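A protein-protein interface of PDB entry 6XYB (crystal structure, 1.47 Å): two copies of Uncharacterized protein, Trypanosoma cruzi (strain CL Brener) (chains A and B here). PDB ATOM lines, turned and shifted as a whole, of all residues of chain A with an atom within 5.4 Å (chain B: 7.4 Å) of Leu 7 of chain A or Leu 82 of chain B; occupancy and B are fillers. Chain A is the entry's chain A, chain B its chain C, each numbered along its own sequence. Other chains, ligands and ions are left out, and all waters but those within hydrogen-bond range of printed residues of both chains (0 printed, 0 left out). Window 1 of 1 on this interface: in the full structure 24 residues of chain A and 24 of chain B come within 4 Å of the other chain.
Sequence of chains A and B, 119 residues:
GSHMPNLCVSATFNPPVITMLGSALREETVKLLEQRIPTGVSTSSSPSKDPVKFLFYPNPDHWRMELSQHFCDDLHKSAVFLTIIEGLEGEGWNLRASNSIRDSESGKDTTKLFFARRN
2 positions are printed for both chains.
The backbone NH of Asn 6 of chain A lies within hydrogen-bond range of the side-chain carboxylate of Glu 86 of chain B (3.0 Å).
NE2 of His 3 of chain A sits at hydrogen-bond distance from O of Thr 83 of chain B (3.2 Å).
The side-chain carboxylate (OE1) of Glu 86 of chain B sits close to the backbone carbonyl oxygen (O) of His 3 of chain A (3.3 Å).
The side-chain hydroxyl (OG1) of Thr 83 of chain B sits at hydrogen-bond distance from the backbone carbonyl oxygen (O) of Val 80 of chain B.
The backbone carbonyl oxygen of Cys 8 of chain A sits at hydrogen-bond distance from the backbone NH of Leu 21 of chain A (2.9 Å).
N of Phe 115 of chain A is in hydrogen-bond range of O of Leu 7 of chain A, 2.8 Å away.
O of Phe 115 of chain A lies close to OD1 of Asn 6 of chain A (3.4 Å).
Among the printed residues, pairs that only touch across the chains: His 3 of chain A with Gly 87 of chain B, Leu 21 of chain A with Leu 82 of chain B, Asn 6 of chain A with Ile 85 of chain B, Leu 21 of chain A with Ala 79 of chain B, Phe 114 of chain A with Ile 85 of chain B, Asn 6 of chain A with Leu 82 of chain B, Cys 8 of chain A with Leu 82 of chain B, Gly 22 of chain A with Leu 82 of chain B, Leu 7 of chain A with Leu 82 of chain B, Leu 21 of chain A with Ser 78 of chain B, Phe 114 of chain A with Phe 81 of chain B and Pro 5 of chain A with Glu 86 of chain B.
Of the printed residues of chain B, Asn 6 of chain A touches Leu 82 (3.6 Å), Ile 85 (3.5 Å) and Glu 86 (3.0 Å).
Of chain B, only Leu 82 (3.8 Å) comes within 4 Å of Leu 7 of chain A.
Leu 25 of chain A touches none of the printed residues of chain B.
Of the printed residues of chain A, Gly 87 of chain B touches His 3.
Leu 113 of chain B touches none of the printed residues of chain A.
The nearest residue of chain A that does not touch Leu 82 of chain B is Phe 114 of chain A (4.7 Å).
The nearest printed residue of chain A that does not touch Gly 87 of chain B is Asn 6 of chain A (6.5 Å).
Hydrophobic or aromatic side chains of chain A that line the printed part of chain B: His 3, Leu 21 and Phe 114.
Among the printed residues, no Asp or Glu carboxylate lies within 4 Å of a Lys or Arg side-chain nitrogen of the other chain.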
ATOM      1  N   HIS A   3     -29.064 -27.731  16.020  1.00  0.00           N
ATOM      2  CA  HIS A   3     -28.067 -26.751  15.560  1.00  0.00           C
ATOM      3  C   HIS A   3     -26.790 -27.587  15.349  1.00  0.00           C
ATOM      4  O   HIS A   3     -26.035 -27.711  16.332  1.00  0.00           O
ATOM      5  CB  HIS A   3     -27.986 -25.667  16.652  1.00  0.00           C
ATOM      6  CG  HIS A   3     -28.270 -24.270  16.202  1.00  0.00           C
ATOM      7  ND1 HIS A   3     -28.963 -23.989  15.034  1.00  0.00           N
ATOM      8  CD2 HIS A   3     -27.988 -23.071  16.778  1.00  0.00           C
ATOM      9  CE1 HIS A   3     -28.972 -22.678  14.844  1.00  0.00           C
ATOM     10  NE2 HIS A   3     -28.456 -22.095  15.925  1.00  0.00           N
ATOM     11  N   PRO A   5     -23.691 -29.923  15.430  1.00  0.00           N
ATOM     12  CA  PRO A   5     -22.922 -29.613  16.628  1.00  0.00           C
ATOM     13  C   PRO A   5     -21.554 -28.952  16.373  1.00  0.00           C
ATOM     14  O   PRO A   5     -20.647 -29.492  15.742  1.00  0.00           O
ATOM     15  CB  PRO A   5     -22.755 -30.962  17.356  1.00  0.00           C
ATOM     16  CG  PRO A   5     -23.107 -32.065  16.315  1.00  0.00           C
ATOM     17  CD  PRO A   5     -23.560 -31.340  15.058  1.00  0.00           C
ATOM     18  N   ASN A   6     -21.456 -27.708  16.822  1.00  0.00           N
ATOM     19  CA  ASN A   6     -20.170 -26.969  16.758  1.00  0.00           C
ATOM     20  C   ASN A   6     -19.754 -26.487  18.153  1.00  0.00           C
ATOM     21  O   ASN A   6     -20.549 -26.409  19.091  1.00  0.00           O
ATOM     22  CB  ASN A   6     -20.318 -25.764  15.837  1.00  0.00           C
ATOM     23  CG  ASN A   6     -20.384 -26.135  14.381  1.00  0.00           C
ATOM     24  OD1 ASN A   6     -19.378 -26.042  13.715  1.00  0.00           O
ATOM     25  ND2 ASN A   6     -21.544 -26.545  13.899  1.00  0.00           N
ATOM     26  N   LEU A   7     -18.501 -26.153  18.289  1.00  0.00           N
ATOM     27  CA  LEU A   7     -17.925 -25.718  19.563  1.00  0.00           C
ATOM     28  C   LEU A   7     -17.142 -24.439  19.267  1.00  0.00           C
ATOM     29  O   LEU A   7     -16.501 -24.347  18.194  1.00  0.00           O
ATOM     30  CB  LEU A   7     -17.085 -26.873  20.125  1.00  0.00           C
ATOM     31  CG  LEU A   7     -16.152 -26.693  21.301  1.00  0.00           C
ATOM     32  CD1 LEU A   7     -16.832 -26.327  22.596  1.00  0.00           C
ATOM     33  CD2 LEU A   7     -15.435 -28.003  21.516  1.00  0.00           C
ATOM     34  N   CYS A   8     -17.149 -23.491  20.219  1.00  0.00           N
ATOM     35  CA  CYS A   8     -16.320 -22.306  20.228  1.00  0.00           C
ATOM     36  C   CYS A   8     -15.527 -22.291  21.514  1.00  0.00           C
ATOM     37  O   CYS A   8     -16.118 -22.358  22.587  1.00  0.00           O
ATOM     38  CB  CYS A   8     -17.047 -21.004  20.042  1.00  0.00           C
ATOM     39  SG  CYS A   8     -16.040 -19.489  20.102  1.00  0.00           S
ATOM     40  N   VAL A   9     -14.212 -22.240  21.397  1.00  0.00           N
ATOM     41  CA  VAL A   9     -13.280 -21.921  22.492  1.00  0.00           C
ATOM     42  C   VAL A   9     -12.719 -20.521  22.312  1.00  0.00           C
ATOM     43  O   VAL A   9     -12.152 -20.243  21.244  1.00  0.00           O
ATOM     44  CB  VAL A   9     -12.166 -22.945  22.709  1.00  0.00           C
ATOM     45  CG1 VAL A   9     -11.393 -22.521  23.945  1.00  0.00           C
ATOM     46  CG2 VAL A   9     -12.758 -24.338  22.854  1.00  0.00           C
ATOM     47  N   MET A  20     -15.580 -21.923  26.975  1.00  0.00           N
ATOM     48  CA  MET A  20     -15.930 -23.027  26.056  1.00  0.00           C
ATOM     49  C   MET A  20     -17.444 -23.080  25.902  1.00  0.00           C
ATOM     50  O   MET A  20     -18.131 -23.181  26.945  1.00  0.00           O
ATOM     51  CB  MET A  20     -15.346 -24.396  26.452  1.00  0.00           C
ATOM     52  CG  MET A  20     -13.797 -24.414  26.831  1.00  0.00           C
ATOM     53  SD  MET A  20     -13.353 -26.159  27.307  1.00  0.00           S
ATOM     54  CE  MET A  20     -13.646 -26.953  25.716  1.00  0.00           C
ATOM     55  N   LEU A  21     -17.945 -23.015  24.674  1.00  0.00           N
ATOM     56  CA  LEU A  21     -19.379 -22.894  24.342  1.00  0.00           C
ATOM     57  C   LEU A  21     -19.684 -23.963  23.320  1.00  0.00           C
ATOM     58  O   LEU A  21     -18.933 -24.146  22.402  1.00  0.00           O
ATOM     59  CB  LEU A  21     -19.669 -21.567  23.640  1.00  0.00           C
ATOM     60  CG  LEU A  21     -19.734 -20.271  24.427  1.00  0.00           C
ATOM     61  CD1 LEU A  21     -18.333 -19.701  24.692  1.00  0.00           C
ATOM     62  CD2 LEU A  21     -20.572 -19.290  23.607  1.00  0.00           C
ATOM     63  N   GLY A  22     -20.814 -24.600  23.461  1.00  0.00           N
ATOM     64  CA  GLY A  22     -21.349 -25.533  22.474  1.00  0.00           C
ATOM     65  C   GLY A  22     -22.377 -26.434  23.138  1.00  0.00           C
ATOM     66  O   GLY A  22     -22.104 -26.997  24.182  1.00  0.00           O
ATOM     67  N   LEU A  25     -21.223 -29.989  24.013  1.00  0.00           N
ATOM     68  CA  LEU A  25     -19.984 -30.125  24.774  1.00  0.00           C
ATOM     69  C   LEU A  25     -20.344 -30.833  26.079  1.00  0.00           C
ATOM     70  O   LEU A  25     -21.229 -30.351  26.771  1.00  0.00           O
ATOM     71  CB  LEU A  25     -19.407 -28.746  25.043  1.00  0.00           C
ATOM     72  CG  LEU A  25     -18.199 -28.650  25.956  1.00  0.00           C
ATOM     73  CD1 LEU A  25     -17.047 -29.434  25.346  1.00  0.00           C
ATOM     74  CD2 LEU A  25     -17.845 -27.185  26.219  1.00  0.00           C
ATOM     75  N   LEU A  88      -9.044 -31.568  22.123  1.00  0.00           N
ATOM     76  CA  LEU A  88     -10.364 -31.611  21.492  1.00  0.00           C
ATOM     77  C   LEU A  88     -10.316 -32.584  20.297  1.00  0.00           C
ATOM     78  O   LEU A  88     -11.350 -33.258  20.039  1.00  0.00           O
ATOM     79  CB  LEU A  88     -10.790 -30.212  21.082  1.00  0.00           C
ATOM     80  CG  LEU A  88     -11.271 -29.381  22.257  1.00  0.00           C
ATOM     81  CD1 LEU A  88     -11.551 -27.945  21.820  1.00  0.00           C
ATOM     82  CD2 LEU A  88     -12.541 -30.004  22.835  1.00  0.00           C
ATOM     83  N   TRP A  93     -13.443 -33.522  18.058  1.00  0.00           N
ATOM     84  CA  TRP A  93     -13.684 -32.111  17.697  1.00  0.00           C
ATOM     85  C   TRP A  93     -12.528 -31.616  16.830  1.00  0.00           C
ATOM     86  O   TRP A  93     -11.421 -31.535  17.349  1.00  0.00           O
ATOM     87  CB  TRP A  93     -13.906 -31.226  18.929  1.00  0.00           C
ATOM     88  CG  TRP A  93     -15.149 -31.491  19.713  1.00  0.00           C
ATOM     89  CD1 TRP A  93     -15.221 -32.067  20.953  1.00  0.00           C
ATOM     90  CD2 TRP A  93     -16.484 -31.088  19.392  1.00  0.00           C
ATOM     91  NE1 TRP A  93     -16.527 -32.128  21.370  1.00  0.00           N
ATOM     92  CE2 TRP A  93     -17.324 -31.516  20.438  1.00  0.00           C
ATOM     93  CE3 TRP A  93     -17.054 -30.433  18.318  1.00  0.00           C
ATOM     94  CZ2 TRP A  93     -18.679 -31.257  20.446  1.00  0.00           C
ATOM     95  CZ3 TRP A  93     -18.386 -30.176  18.300  1.00  0.00           C
ATOM     96  CH2 TRP A  93     -19.185 -30.575  19.376  1.00  0.00           C
ATOM     97  N   LEU A 113     -11.439 -20.104  18.614  1.00  0.00           N
ATOM     98  CA  LEU A 113     -11.218 -21.361  17.892  1.00  0.00           C
ATOM     99  C   LEU A 113     -12.563 -22.010  17.652  1.00  0.00           C
ATOM    100  O   LEU A 113     -13.297 -22.201  18.645  1.00  0.00           O
ATOM    101  CB  LEU A 113     -10.276 -22.301  18.657  1.00  0.00           C
ATOM    102  CG  LEU A 113      -8.897 -21.759  19.054  1.00  0.00           C
ATOM    103  CD1 LEU A 113      -8.211 -22.590  20.143  1.00  0.00           C
ATOM    104  CD2 LEU A 113      -7.981 -21.732  17.862  1.00  0.00           C
ATOM    105  N   PHE A 114     -12.866 -22.414  16.441  1.00  0.00           N
ATOM    106  CA  PHE A 114     -14.149 -23.016  16.052  1.00  0.00           C
ATOM    107  C   PHE A 114     -13.939 -24.473  15.632  1.00  0.00           C
ATOM    108  O   PHE A 114     -13.053 -24.728  14.782  1.00  0.00           O
ATOM    109  CB  PHE A 114     -14.807 -22.231  14.922  1.00  0.00           C
ATOM    110  CG  PHE A 114     -15.141 -20.812  15.288  1.00  0.00           C
ATOM    111  CD1 PHE A 114     -16.272 -20.521  16.040  1.00  0.00           C
ATOM    112  CD2 PHE A 114     -14.255 -19.823  14.970  1.00  0.00           C
ATOM    113  CE1 PHE A 114     -16.542 -19.226  16.410  1.00  0.00           C
ATOM    114  CE2 PHE A 114     -14.509 -18.502  15.352  1.00  0.00           C
ATOM    115  CZ  PHE A 114     -15.679 -18.210  16.035  1.00  0.00           C
ATOM    116  N   PHE A 115     -14.725 -25.387  16.236  1.00  0.00           N
ATOM    117  CA  PHE A 115     -14.588 -26.835  16.029  1.00  0.00           C
ATOM    118  C   PHE A 115     -15.885 -27.458  15.566  1.00  0.00           C
ATOM    119  O   PHE A 115     -16.975 -26.983  15.900  1.00  0.00           O
ATOM    120  CB  PHE A 115     -14.123 -27.554  17.287  1.00  0.00           C
ATOM    121  CG  PHE A 115     -12.867 -27.060  17.903  1.00  0.00           C
ATOM    122  CD1 PHE A 115     -12.880 -25.911  18.683  1.00  0.00           C
ATOM    123  CD2 PHE A 115     -11.677 -27.734  17.687  1.00  0.00           C
ATOM    124  CE1 PHE A 115     -11.704 -25.417  19.213  1.00  0.00           C
ATOM    125  CE2 PHE A 115     -10.499 -27.239  18.225  1.00  0.00           C
ATOM    126  CZ  PHE A 115     -10.526 -26.103  18.994  1.00  0.00           C
ATOM    127  N   ALA A 116     -15.747 -28.539  14.835  1.00  0.00           N
ATOM    128  CA  ALA A 116     -16.901 -29.346  14.378  1.00  0.00           C
ATOM    129  C   ALA A 116     -16.588 -30.807  14.536  1.00  0.00           C
ATOM    130  O   ALA A 116     -15.462 -31.211  14.661  1.00  0.00           O
ATOM    131  CB  ALA A 116     -17.242 -29.032  12.951  1.00  0.00           C
ATOM    132  N   HIS B  76     -21.028 -13.076  24.680  1.00  0.00           N
ATOM    133  CA  HIS B  76     -22.235 -13.046  23.834  1.00  0.00           C
ATOM    134  C   HIS B  76     -21.824 -13.028  22.351  1.00  0.00           C
ATOM    135  O   HIS B  76     -22.580 -13.562  21.506  1.00  0.00           O
ATOM    136  CB  HIS B  76     -23.160 -11.907  24.262  1.00  0.00           C
ATOM    137  CG  HIS B  76     -23.978 -12.280  25.454  1.00  0.00           C
ATOM    138  ND1 HIS B  76     -23.437 -12.383  26.728  1.00  0.00           N
ATOM    139  CD2 HIS B  76     -25.273 -12.665  25.558  1.00  0.00           C
ATOM    140  CE1 HIS B  76     -24.388 -12.750  27.593  1.00  0.00           C
ATOM    141  NE2 HIS B  76     -25.527 -12.938  26.903  1.00  0.00           N
ATOM    142  N   LYS B  77     -20.672 -12.438  22.032  1.00  0.00           N
ATOM    143  CA  LYS B  77     -20.178 -12.416  20.651  1.00  0.00           C
ATOM    144  C   LYS B  77     -19.883 -13.887  20.246  1.00  0.00           C
ATOM    145  O   LYS B  77     -20.282 -14.302  19.183  1.00  0.00           O
ATOM    146  CB  LYS B  77     -18.908 -11.585  20.574  1.00  0.00           C
ATOM    147  CG  LYS B  77     -19.109 -10.116  20.863  1.00  0.00           C
ATOM    148  CD  LYS B  77     -17.851  -9.318  20.781  1.00  0.00           C
ATOM    149  CE  LYS B  77     -17.921  -7.996  21.533  1.00  0.00           C
ATOM    150  NZ  LYS B  77     -16.609  -7.299  21.538  1.00  0.00           N
ATOM    151  N   SER B  78     -19.233 -14.688  21.107  1.00  0.00           N
ATOM    152  CA  SER B  78     -18.942 -16.109  20.829  1.00  0.00           C
ATOM    153  C   SER B  78     -20.268 -16.820  20.555  1.00  0.00           C
ATOM    154  O   SER B  78     -20.340 -17.640  19.661  1.00  0.00           O
ATOM    155  CB  SER B  78     -18.206 -16.714  22.017  1.00  0.00           C
ATOM    156  OG  SER B  78     -16.931 -16.111  22.231  1.00  0.00           O
ATOM    157  N   ALA B  79     -21.271 -16.560  21.394  1.00  0.00           N
ATOM    158  CA  ALA B  79     -22.582 -17.204  21.217  1.00  0.00           C
ATOM    159  C   ALA B  79     -23.221 -16.830  19.863  1.00  0.00           C
ATOM    160  O   ALA B  79     -23.822 -17.668  19.231  1.00  0.00           O
ATOM    161  CB  ALA B  79     -23.499 -16.802  22.362  1.00  0.00           C
ATOM    162  N   VAL B  80     -23.170 -15.593  19.469  1.00  0.00           N
ATOM    163  CA  VAL B  80     -23.748 -15.171  18.155  1.00  0.00           C
ATOM    164  C   VAL B  80     -23.019 -15.917  17.041  1.00  0.00           C
ATOM    165  O   VAL B  80     -23.640 -16.461  16.101  1.00  0.00           O
ATOM    166  CB  VAL B  80     -23.604 -13.666  17.950  1.00  0.00           C
ATOM    167  CG1 VAL B  80     -23.921 -13.285  16.521  1.00  0.00           C
ATOM    168  CG2 VAL B  80     -24.481 -12.892  18.936  1.00  0.00           C
ATOM    169  N   PHE B  81     -21.712 -15.968  17.126  1.00  0.00           N
ATOM    170  CA  PHE B  81     -20.966 -16.655  16.026  1.00  0.00           C
ATOM    171  C   PHE B  81     -21.370 -18.132  15.995  1.00  0.00           C
ATOM    172  O   PHE B  81     -21.592 -18.674  14.883  1.00  0.00           O
ATOM    173  CB  PHE B  81     -19.452 -16.616  16.238  1.00  0.00           C
ATOM    174  CG  PHE B  81     -18.886 -15.219  16.295  1.00  0.00           C
ATOM    175  CD1 PHE B  81     -19.420 -14.198  15.538  1.00  0.00           C
ATOM    176  CD2 PHE B  81     -17.777 -14.929  17.077  1.00  0.00           C
ATOM    177  CE1 PHE B  81     -18.869 -12.922  15.602  1.00  0.00           C
ATOM    178  CE2 PHE B  81     -17.220 -13.665  17.119  1.00  0.00           C
ATOM    179  CZ  PHE B  81     -17.812 -12.641  16.431  1.00  0.00           C
ATOM    180  N   LEU B  82     -21.368 -18.820  17.163  1.00  0.00           N
ATOM    181  CA  LEU B  82     -21.754 -20.252  17.161  1.00  0.00           C
ATOM    182  C   LEU B  82     -23.152 -20.474  16.572  1.00  0.00           C
ATOM    183  O   LEU B  82     -23.381 -21.443  15.816  1.00  0.00           O
ATOM    184  CB  LEU B  82     -21.701 -20.848  18.577  1.00  0.00           C
ATOM    185  CG  LEU B  82     -20.520 -21.749  18.862  1.00  0.00           C
ATOM    186  CD1 LEU B  82     -20.767 -22.548  20.134  1.00  0.00           C
ATOM    187  CD2 LEU B  82     -20.158 -22.654  17.695  1.00  0.00           C
ATOM    188  N   THR B  83     -24.111 -19.633  16.944  1.00  0.00           N
ATOM    189  CA  THR B  83     -25.511 -19.864  16.486  1.00  0.00           C
ATOM    190  C   THR B  83     -25.584 -19.626  14.962  1.00  0.00           C
ATOM    191  O   THR B  83     -26.273 -20.373  14.298  1.00  0.00           O
ATOM    192  CB  THR B  83     -26.583 -19.094  17.282  1.00  0.00           C
ATOM    193  OG1 THR B  83     -26.545 -17.691  16.993  1.00  0.00           O
ATOM    194  CG2 THR B  83     -26.499 -19.292  18.782  1.00  0.00           C
ATOM    195  N   ILE B  84     -24.849 -18.641  14.435  1.00  0.00           N
ATOM    196  CA  ILE B  84     -24.786 -18.421  12.961  1.00  0.00           C
ATOM    197  C   ILE B  84     -24.194 -19.672  12.309  1.00  0.00           C
ATOM    198  O   ILE B  84     -24.717 -20.128  11.290  1.00  0.00           O
ATOM    199  CB  ILE B  84     -24.013 -17.138  12.598  1.00  0.00           C
ATOM    200  CG1 ILE B  84     -24.723 -15.882  13.135  1.00  0.00           C
ATOM    201  CG2 ILE B  84     -23.674 -17.119  11.095  1.00  0.00           C
ATOM    202  CD1 ILE B  84     -23.844 -14.660  13.088  1.00  0.00           C
ATOM    203  N   ILE B  85     -23.069 -20.136  12.837  1.00  0.00           N
ATOM    204  CA  ILE B  85     -22.383 -21.296  12.175  1.00  0.00           C
ATOM    205  C   ILE B  85     -23.328 -22.504  12.216  1.00  0.00           C
ATOM    206  O   ILE B  85     -23.454 -23.216  11.235  1.00  0.00           O
ATOM    207  CB  ILE B  85     -21.048 -21.608  12.850  1.00  0.00           C
ATOM    208  CG1 ILE B  85     -20.076 -20.434  12.638  1.00  0.00           C
ATOM    209  CG2 ILE B  85     -20.490 -22.964  12.413  1.00  0.00           C
ATOM    210  CD1 ILE B  85     -18.971 -20.353  13.646  1.00  0.00           C
ATOM    211  N   GLU B  86     -23.903 -22.776  13.368  1.00  0.00           N
ATOM    212  CA  GLU B  86     -24.771 -23.956  13.567  1.00  0.00           C
ATOM    213  C   GLU B  86     -25.987 -23.859  12.638  1.00  0.00           C
ATOM    214  O   GLU B  86     -26.346 -24.818  11.931  1.00  0.00           O
ATOM    215  CB  GLU B  86     -25.173 -24.055  15.051  1.00  0.00           C
ATOM    216  CG  GLU B  86     -24.060 -24.630  15.873  1.00  0.00           C
ATOM    217  CD  GLU B  86     -24.451 -25.101  17.238  1.00  0.00           C
ATOM    218  OE1 GLU B  86     -25.565 -24.703  17.670  1.00  0.00           O
ATOM    219  OE2 GLU B  86     -23.654 -25.911  17.817  1.00  0.00           O
ATOM    220  N   GLY B  87     -26.550 -22.688  12.567  1.00  0.00           N
ATOM    221  CA  GLY B  87     -27.750 -22.519  11.748  1.00  0.00           C
ATOM    222  C   GLY B  87     -27.473 -22.690  10.264  1.00  0.00           C
ATOM    223  O   GLY B  87     -28.218 -23.359   9.536  1.00  0.00           O
ATOM    224  N   LEU B  88     -26.383 -22.084   9.801  1.00  0.00           N
ATOM    225  CA  LEU B  88     -25.971 -22.225   8.399  1.00  0.00           C
ATOM    226  C   LEU B  88     -25.546 -23.659   8.105  1.00  0.00           C
ATOM    227  O   LEU B  88     -25.809 -24.094   6.944  1.00  0.00           O
ATOM    228  CB  LEU B  88     -24.911 -21.191   8.088  1.00  0.00           C
ATOM    229  CG  LEU B  88     -25.411 -19.761   8.011  1.00  0.00           C
ATOM    230  CD1 LEU B  88     -24.220 -18.804   7.901  1.00  0.00           C
ATOM    231  CD2 LEU B  88     -26.332 -19.611   6.831  1.00  0.00           C
ATOM    232  N   LEU B 113     -17.014 -14.345   8.646  1.00  0.00           N
ATOM    233  CA  LEU B 113     -17.154 -15.811   8.595  1.00  0.00           C
ATOM    234  C   LEU B 113     -17.449 -16.110   7.118  1.00  0.00           C
ATOM    235  O   LEU B 113     -18.447 -15.555   6.539  1.00  0.00           O
ATOM    236  CB  LEU B 113     -18.281 -16.264   9.519  1.00  0.00           C
ATOM    237  CG  LEU B 113     -18.148 -16.024  11.013  1.00  0.00           C
ATOM    238  CD1 LEU B 113     -19.515 -16.193  11.694  1.00  0.00           C
ATOM    239  CD2 LEU B 113     -17.201 -17.015  11.694  1.00  0.00           C
